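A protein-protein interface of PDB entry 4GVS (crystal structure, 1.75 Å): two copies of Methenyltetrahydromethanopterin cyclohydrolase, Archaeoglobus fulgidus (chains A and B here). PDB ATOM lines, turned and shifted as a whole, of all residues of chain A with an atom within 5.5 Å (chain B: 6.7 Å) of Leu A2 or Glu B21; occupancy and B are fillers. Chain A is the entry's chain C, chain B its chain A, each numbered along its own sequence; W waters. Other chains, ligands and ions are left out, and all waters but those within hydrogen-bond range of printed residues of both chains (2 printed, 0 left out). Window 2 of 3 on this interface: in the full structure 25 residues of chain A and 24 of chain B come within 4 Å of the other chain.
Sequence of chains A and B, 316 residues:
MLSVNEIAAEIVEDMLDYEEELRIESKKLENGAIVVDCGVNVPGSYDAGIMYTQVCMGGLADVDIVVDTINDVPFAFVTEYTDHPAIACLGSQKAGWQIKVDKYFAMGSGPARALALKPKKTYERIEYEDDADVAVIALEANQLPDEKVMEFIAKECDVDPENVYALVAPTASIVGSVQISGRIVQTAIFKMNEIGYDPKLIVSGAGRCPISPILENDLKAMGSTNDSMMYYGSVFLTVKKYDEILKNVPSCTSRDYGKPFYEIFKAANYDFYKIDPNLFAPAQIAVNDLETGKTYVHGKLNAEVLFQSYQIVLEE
Leu A2 touches Glu B20. Leu A2 touches Glu B21. Asp A83 touches Ser B45. Glu B20 touches His A84. O of Glu B21 touches CE1 of His A84, at 3.2 Å.
Of the printed residues of chain B, Met A1 touches Glu B20. Leu A2 touches two residues of chain B. Of the printed residues of chain B, His A84 touches Glu B20, Glu B21 and Arg B23. Glu B21 touches just these residues of chain A: Leu A2 (3.7 Å) and His A84 (3.2 Å). Asp B47 touches none of the printed residues of chain A. The nearest residue of chain A that does not touch Glu B21 is Ile A7 (4.5 Å).
Water W2 bridges O of Glu B20 (2.6 Å) and NE2 of His A84 (2.8 Å). Water W1 lies within hydrogen-bond range of O of Asp A83 (3.2 Å) and NH2 of Arg B23 (3.2 Å).
No position is printed for both chains. Of the 8 pairs that touch across the chains among the printed residues, none has its exchanged pair printed and touching as well.
A ring nitrogen (NE2) of His A84 lies within hydrogen-bond range of the guanidinium group (NE) of Arg B23 (3.4 Å). O of Asp A83 is in hydrogen-bond range of NE of Arg B23 (2.8 Å). The backbone NH (N) of Met A1 is in hydrogen-bond range of the side-chain carboxylate (OE2) of Glu B20.
Along chain A the printed residues that touch a printed residue of chain B span positions 1 to 84. Of the 11 printed residues of chain B, 4 touch a printed residue of chain A. Printed residues of chain B that touch a printed residue of chain A: Glu B20, Glu B21, Arg B23 and Ser B45. Along chain B the printed residues that touch a printed residue of chain A span positions 20 to 45. Among the printed residues, 8 pairs touch across the chains. Among the printed residues, no Asp or Glu carboxylate lies within 4 Å of a Lys or Arg side-chain nitrogen of the other chain.
The side-chain hydroxyl (OH) of Tyr A128 sits at hydrogen-bond distance from the backbone carbonyl oxygen (O) of Leu A2, at 2.6 Å. The backbone carbonyl oxygen (O) of Leu B22 lies within hydrogen-bond range of the side-chain hydroxyl (OG) of Ser B45, 2.6 Å away. The backbone NH (N) of Gly B44 sits at hydrogen-bond distance from the backbone carbonyl oxygen (O) of Arg B23.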
ATOM      1  N   MET A   1       7.749 -21.341  -3.674  1.00  0.00           N
ATOM      2  CA  MET A   1       7.568 -22.722  -4.116  1.00  0.00           C
ATOM      3  C   MET A   1       6.102 -23.110  -4.096  1.00  0.00           C
ATOM      4  O   MET A   1       5.800 -24.294  -4.115  1.00  0.00           O
ATOM      5  CB  MET A   1       8.324 -23.705  -3.206  1.00  0.00           C
ATOM      6  CG  MET A   1       8.683 -24.993  -3.985  1.00  0.00           C
ATOM      7  SD  MET A   1       8.524 -26.612  -3.161  1.00  0.00           S
ATOM      8  CE  MET A   1       8.362 -27.746  -4.544  1.00  0.00           C
ATOM      9  N   LEU A   2       5.188 -22.158  -3.986  1.00  0.00           N
ATOM     10  CA  LEU A   2       3.761 -22.529  -4.133  1.00  0.00           C
ATOM     11  C   LEU A   2       3.307 -22.256  -5.575  1.00  0.00           C
ATOM     12  O   LEU A   2       3.427 -21.120  -6.000  1.00  0.00           O
ATOM     13  CB  LEU A   2       2.882 -21.680  -3.178  1.00  0.00           C
ATOM     14  CG  LEU A   2       3.171 -21.884  -1.667  1.00  0.00           C
ATOM     15  CD1 LEU A   2       2.406 -20.871  -0.838  1.00  0.00           C
ATOM     16  CD2 LEU A   2       2.828 -23.292  -1.242  1.00  0.00           C
ATOM     17  N   SER A   3       2.763 -23.258  -6.268  1.00  0.00           N
ATOM     18  CA  SER A   3       2.251 -23.045  -7.635  1.00  0.00           C
ATOM     19  C   SER A   3       0.743 -22.867  -7.603  1.00  0.00           C
ATOM     20  O   SER A   3       0.033 -23.835  -7.390  1.00  0.00           O
ATOM     21  CB  SER A   3       2.608 -24.244  -8.516  1.00  0.00           C
ATOM     22  OG  SER A   3       2.022 -24.123  -9.810  1.00  0.00           O
ATOM     23  N   VAL A   4       0.250 -21.641  -7.816  1.00  0.00           N
ATOM     24  CA  VAL A   4      -1.222 -21.444  -7.794  1.00  0.00           C
ATOM     25  C   VAL A   4      -1.881 -22.285  -8.875  1.00  0.00           C
ATOM     26  O   VAL A   4      -2.995 -22.760  -8.707  1.00  0.00           O
ATOM     27  CB  VAL A   4      -1.598 -19.951  -7.868  1.00  0.00           C
ATOM     28  CG1 VAL A   4      -1.212 -19.231  -6.556  1.00  0.00           C
ATOM     29  CG2 VAL A   4      -0.897 -19.256  -9.051  1.00  0.00           C
ATOM     30  N   ILE A   7      -1.920 -26.075  -7.721  1.00  0.00           N
ATOM     31  CA  ILE A   7      -2.812 -26.293  -6.582  1.00  0.00           C
ATOM     32  C   ILE A   7      -4.282 -26.204  -7.073  1.00  0.00           C
ATOM     33  O   ILE A   7      -5.169 -27.070  -6.719  1.00  0.00           O
ATOM     34  CB  ILE A   7      -2.519 -25.278  -5.469  1.00  0.00           C
ATOM     35  CG1 ILE A   7      -1.110 -25.504  -4.878  1.00  0.00           C
ATOM     36  CG2 ILE A   7      -3.562 -25.356  -4.316  1.00  0.00           C
ATOM     37  CD1 ILE A   7      -0.689 -24.317  -4.010  1.00  0.00           C
ATOM     38  N   LEU A  60      -5.078 -20.930  -2.109  1.00  0.00           N
ATOM     39  CA  LEU A  60      -4.360 -20.388  -0.980  1.00  0.00           C
ATOM     40  C   LEU A  60      -5.313 -19.661  -0.010  1.00  0.00           C
ATOM     41  O   LEU A  60      -4.876 -18.876   0.831  1.00  0.00           O
ATOM     42  CB  LEU A  60      -3.247 -19.436  -1.429  1.00  0.00           C
ATOM     43  CG  LEU A  60      -2.182 -20.118  -2.306  1.00  0.00           C
ATOM     44  CD1 LEU A  60      -1.044 -19.109  -2.600  1.00  0.00           C
ATOM     45  CD2 LEU A  60      -1.606 -21.308  -1.497  1.00  0.00           C
ATOM     46  N   ASP A  83      -3.770 -16.414   4.268  1.00  0.00           N
ATOM     47  CA  ASP A  83      -2.500 -15.900   4.779  1.00  0.00           C
ATOM     48  C   ASP A  83      -1.494 -15.661   3.636  1.00  0.00           C
ATOM     49  O   ASP A  83      -0.292 -15.543   3.882  1.00  0.00           O
ATOM     50  CB  ASP A  83      -1.934 -16.884   5.789  1.00  0.00           C
ATOM     51  CG  ASP A  83      -2.636 -16.736   7.138  1.00  0.00           C
ATOM     52  OD1 ASP A  83      -3.663 -17.425   7.330  1.00  0.00           O
ATOM     53  OD2 ASP A  83      -2.226 -15.891   7.922  1.00  0.00           O
ATOM     54  N   HIS A  84      -1.984 -15.645   2.407  1.00  0.00           N
ATOM     55  CA  HIS A  84      -1.196 -15.231   1.253  1.00  0.00           C
ATOM     56  C   HIS A  84      -1.992 -14.178   0.458  1.00  0.00           C
ATOM     57  O   HIS A  84      -2.283 -14.402  -0.758  1.00  0.00           O
ATOM     58  CB  HIS A  84      -0.910 -16.436   0.371  1.00  0.00           C
ATOM     59  CG  HIS A  84      -0.006 -17.437   0.997  1.00  0.00           C
ATOM     60  ND1 HIS A  84      -0.452 -18.416   1.823  1.00  0.00           N
ATOM     61  CD2 HIS A  84       1.392 -17.518   1.000  1.00  0.00           C
ATOM     62  CE1 HIS A  84       0.605 -19.137   2.269  1.00  0.00           C
ATOM     63  NE2 HIS A  84       1.728 -18.572   1.784  1.00  0.00           N
ATOM     64  N   TYR A 128       6.103 -12.496  -7.129  1.00  0.00           N
ATOM     65  CA  TYR A 128       5.636 -13.853  -7.356  1.00  0.00           C
ATOM     66  C   TYR A 128       5.527 -14.082  -8.816  1.00  0.00           C
ATOM     67  O   TYR A 128       4.947 -13.263  -9.483  1.00  0.00           O
ATOM     68  CB  TYR A 128       4.223 -14.099  -6.701  1.00  0.00           C
ATOM     69  CG  TYR A 128       3.752 -15.530  -6.975  1.00  0.00           C
ATOM     70  CD1 TYR A 128       4.293 -16.612  -6.258  1.00  0.00           C
ATOM     71  CD2 TYR A 128       2.774 -15.811  -7.953  1.00  0.00           C
ATOM     72  CE1 TYR A 128       3.878 -17.939  -6.542  1.00  0.00           C
ATOM     73  CE2 TYR A 128       2.339 -17.102  -8.229  1.00  0.00           C
ATOM     74  CZ  TYR A 128       2.891 -18.173  -7.509  1.00  0.00           C
ATOM     75  OH  TYR A 128       2.459 -19.482  -7.769  1.00  0.00           O
ATOM     76  N   ASP A 130       4.449 -17.831 -11.161  1.00  0.00           N
ATOM     77  CA  ASP A 130       4.260 -19.238 -11.127  1.00  0.00           C
ATOM     78  C   ASP A 130       5.158 -19.909 -12.156  1.00  0.00           C
ATOM     79  O   ASP A 130       5.600 -19.273 -13.126  1.00  0.00           O
ATOM     80  CB  ASP A 130       2.803 -19.621 -11.391  1.00  0.00           C
ATOM     81  CG  ASP A 130       2.454 -21.028 -10.902  1.00  0.00           C
ATOM     82  OD1 ASP A 130       3.311 -21.862 -10.441  1.00  0.00           O
ATOM     83  OD2 ASP A 130       1.252 -21.318 -10.996  1.00  0.00           O
ATOM     84  N   ASP B  17       2.809 -31.989   5.724  1.00  0.00           N
ATOM     85  CA  ASP B  17       2.677 -32.095   4.269  1.00  0.00           C
ATOM     86  C   ASP B  17       2.364 -30.751   3.616  1.00  0.00           C
ATOM     87  O   ASP B  17       2.405 -30.639   2.397  1.00  0.00           O
ATOM     88  CB  ASP B  17       1.574 -33.052   3.864  1.00  0.00           C
ATOM     89  CG  ASP B  17       1.926 -34.513   4.134  1.00  0.00           C
ATOM     90  OD1 ASP B  17       3.112 -34.834   4.252  1.00  0.00           O
ATOM     91  OD2 ASP B  17       0.966 -35.290   4.212  1.00  0.00           O
ATOM     92  N   TYR B  18       2.037 -29.761   4.433  1.00  0.00           N
ATOM     93  CA  TYR B  18       1.620 -28.448   3.884  1.00  0.00           C
ATOM     94  C   TYR B  18       2.339 -27.304   4.554  1.00  0.00           C
ATOM     95  O   TYR B  18       1.776 -26.231   4.739  1.00  0.00           O
ATOM     96  CB  TYR B  18       0.072 -28.291   4.058  1.00  0.00           C
ATOM     97  CG  TYR B  18      -0.686 -29.204   3.162  1.00  0.00           C
ATOM     98  CD1 TYR B  18      -0.950 -28.864   1.836  1.00  0.00           C
ATOM     99  CD2 TYR B  18      -1.100 -30.476   3.624  1.00  0.00           C
ATOM    100  CE1 TYR B  18      -1.603 -29.747   0.973  1.00  0.00           C
ATOM    101  CE2 TYR B  18      -1.751 -31.345   2.781  1.00  0.00           C
ATOM    102  CZ  TYR B  18      -2.023 -30.970   1.460  1.00  0.00           C
ATOM    103  OH  TYR B  18      -2.680 -31.859   0.624  1.00  0.00           O
ATOM    104  N   GLU B  19       3.642 -27.475   4.851  1.00  0.00           N
ATOM    105  CA  GLU B  19       4.355 -26.460   5.592  1.00  0.00           C
ATOM    106  C   GLU B  19       4.366 -25.088   4.950  1.00  0.00           C
ATOM    107  O   GLU B  19       4.173 -24.077   5.615  1.00  0.00           O
ATOM    108  CB  GLU B  19       5.822 -26.939   5.810  1.00  0.00           C
ATOM    109  CG  GLU B  19       5.812 -28.160   6.727  1.00  0.00           C
ATOM    110  CD  GLU B  19       7.214 -28.399   7.318  1.00  0.00           C
ATOM    111  OE1 GLU B  19       8.089 -27.517   7.217  1.00  0.00           O
ATOM    112  OE2 GLU B  19       7.405 -29.459   7.849  1.00  0.00           O
ATOM    113  N   GLU B  20       4.633 -25.046   3.648  1.00  0.00           N
ATOM    114  CA  GLU B  20       4.792 -23.758   3.006  1.00  0.00           C
ATOM    115  C   GLU B  20       3.456 -23.029   2.945  1.00  0.00           C
ATOM    116  O   GLU B  20       3.401 -21.833   3.215  1.00  0.00           O
ATOM    117  CB  GLU B  20       5.379 -23.918   1.598  1.00  0.00           C
ATOM    118  CG  GLU B  20       5.862 -22.565   1.044  1.00  0.00           C
ATOM    119  CD  GLU B  20       6.710 -22.704  -0.245  1.00  0.00           C
ATOM    120  OE1 GLU B  20       6.947 -23.817  -0.733  1.00  0.00           O
ATOM    121  OE2 GLU B  20       7.076 -21.660  -0.768  1.00  0.00           O
ATOM    122  N   GLU B  21       2.399 -23.767   2.615  1.00  0.00           N
ATOM    123  CA  GLU B  21       1.022 -23.242   2.589  1.00  0.00           C
ATOM    124  C   GLU B  21       0.626 -22.720   3.959  1.00  0.00           C
ATOM    125  O   GLU B  21       0.008 -21.670   4.071  1.00  0.00           O
ATOM    126  CB  GLU B  21       0.017 -24.349   2.213  1.00  0.00           C
ATOM    127  CG  GLU B  21       0.152 -24.905   0.788  1.00  0.00           C
ATOM    128  CD  GLU B  21       1.171 -26.062   0.549  1.00  0.00           C
ATOM    129  OE1 GLU B  21       2.150 -26.335   1.372  1.00  0.00           O
ATOM    130  OE2 GLU B  21       0.994 -26.711  -0.547  1.00  0.00           O
ATOM    131  N   LEU B  22       1.004 -23.445   5.025  1.00  0.00           N
ATOM    132  CA  LEU B  22       0.587 -23.047   6.385  1.00  0.00           C
ATOM    133  C   LEU B  22       1.530 -21.973   7.025  1.00  0.00           C
ATOM    134  O   LEU B  22       1.258 -21.435   8.086  1.00  0.00           O
ATOM    135  CB  LEU B  22       0.651 -24.311   7.262  1.00  0.00           C
ATOM    136  CG  LEU B  22      -0.451 -25.353   6.894  1.00  0.00           C
ATOM    137  CD1 LEU B  22      -0.203 -26.663   7.633  1.00  0.00           C
ATOM    138  CD2 LEU B  22      -1.835 -24.790   7.287  1.00  0.00           C
ATOM    139  N   ARG B  23       2.619 -21.712   6.300  1.00  0.00           N
ATOM    140  CA  ARG B  23       3.684 -20.790   6.691  1.00  0.00           C
ATOM    141  C   ARG B  23       4.297 -21.186   8.046  1.00  0.00           C
ATOM    142  O   ARG B  23       4.509 -20.348   8.928  1.00  0.00           O
ATOM    143  CB  ARG B  23       3.213 -19.323   6.700  1.00  0.00           C
ATOM    144  CG  ARG B  23       2.496 -18.808   5.444  1.00  0.00           C
ATOM    145  CD  ARG B  23       2.644 -17.257   5.527  1.00  0.00           C
ATOM    146  NE  ARG B  23       2.302 -16.445   4.381  1.00  0.00           N
ATOM    147  CZ  ARG B  23       3.166 -15.977   3.468  1.00  0.00           C
ATOM    148  NH1 ARG B  23       4.460 -16.262   3.497  1.00  0.00           N
ATOM    149  NH2 ARG B  23       2.711 -15.222   2.506  1.00  0.00           N
ATOM    150  N   ILE B  24       4.585 -22.479   8.158  1.00  0.00           N
ATOM    151  CA  ILE B  24       5.307 -23.037   9.295  1.00  0.00           C
ATOM    152  C   ILE B  24       6.599 -23.707   8.815  1.00  0.00           C
ATOM    153  O   ILE B  24       6.795 -23.927   7.626  1.00  0.00           O
ATOM    154  CB  ILE B  24       4.422 -24.039  10.074  1.00  0.00           C
ATOM    155  CG1 ILE B  24       4.069 -25.258   9.188  1.00  0.00           C
ATOM    156  CG2 ILE B  24       3.213 -23.316  10.639  1.00  0.00           C
ATOM    157  CD1 ILE B  24       3.211 -26.355   9.839  1.00  0.00           C
ATOM    158  N   GLY B  44       3.280 -18.395  10.645  1.00  0.00           N
ATOM    159  CA  GLY B  44       2.095 -19.291  10.820  1.00  0.00           C
ATOM    160  C   GLY B  44       0.898 -18.716  10.037  1.00  0.00           C
ATOM    161  O   GLY B  44       1.077 -17.891   9.111  1.00  0.00           O
ATOM    162  N   SER B  45      -0.306 -19.118  10.421  1.00  0.00           N
ATOM    163  CA  SER B  45      -1.498 -18.857   9.561  1.00  0.00           C
ATOM    164  C   SER B  45      -2.712 -19.194  10.342  1.00  0.00           C
ATOM    165  O   SER B  45      -2.628 -19.894  11.361  1.00  0.00           O
ATOM    166  CB  SER B  45      -1.462 -19.714   8.286  1.00  0.00           C
ATOM    167  OG  SER B  45      -1.324 -21.116   8.539  1.00  0.00           O
ATOM    168  N   ASP B  47      -4.973 -21.306   9.334  1.00  0.00           N
ATOM    169  CA  ASP B  47      -5.120 -22.749   9.256  1.00  0.00           C
ATOM    170  C   ASP B  47      -4.125 -23.480  10.152  1.00  0.00           C
ATOM    171  O   ASP B  47      -4.477 -24.502  10.788  1.00  0.00           O
ATOM    172  CB  ASP B  47      -4.988 -23.227   7.832  1.00  0.00           C
ATOM    173  CG  ASP B  47      -6.318 -23.119   7.077  1.00  0.00           C
ATOM    174  OD1 ASP B  47      -7.351 -23.014   7.745  1.00  0.00           O
ATOM    175  OD2 ASP B  47      -6.270 -23.305   5.869  1.00  0.00           O
HETATM  176  O   HOH W   1       1.146 -12.674   3.727  1.00  0.00           O
HETATM  177  O   HOH W   2       4.294 -19.543   2.245  1.00  0.00           O
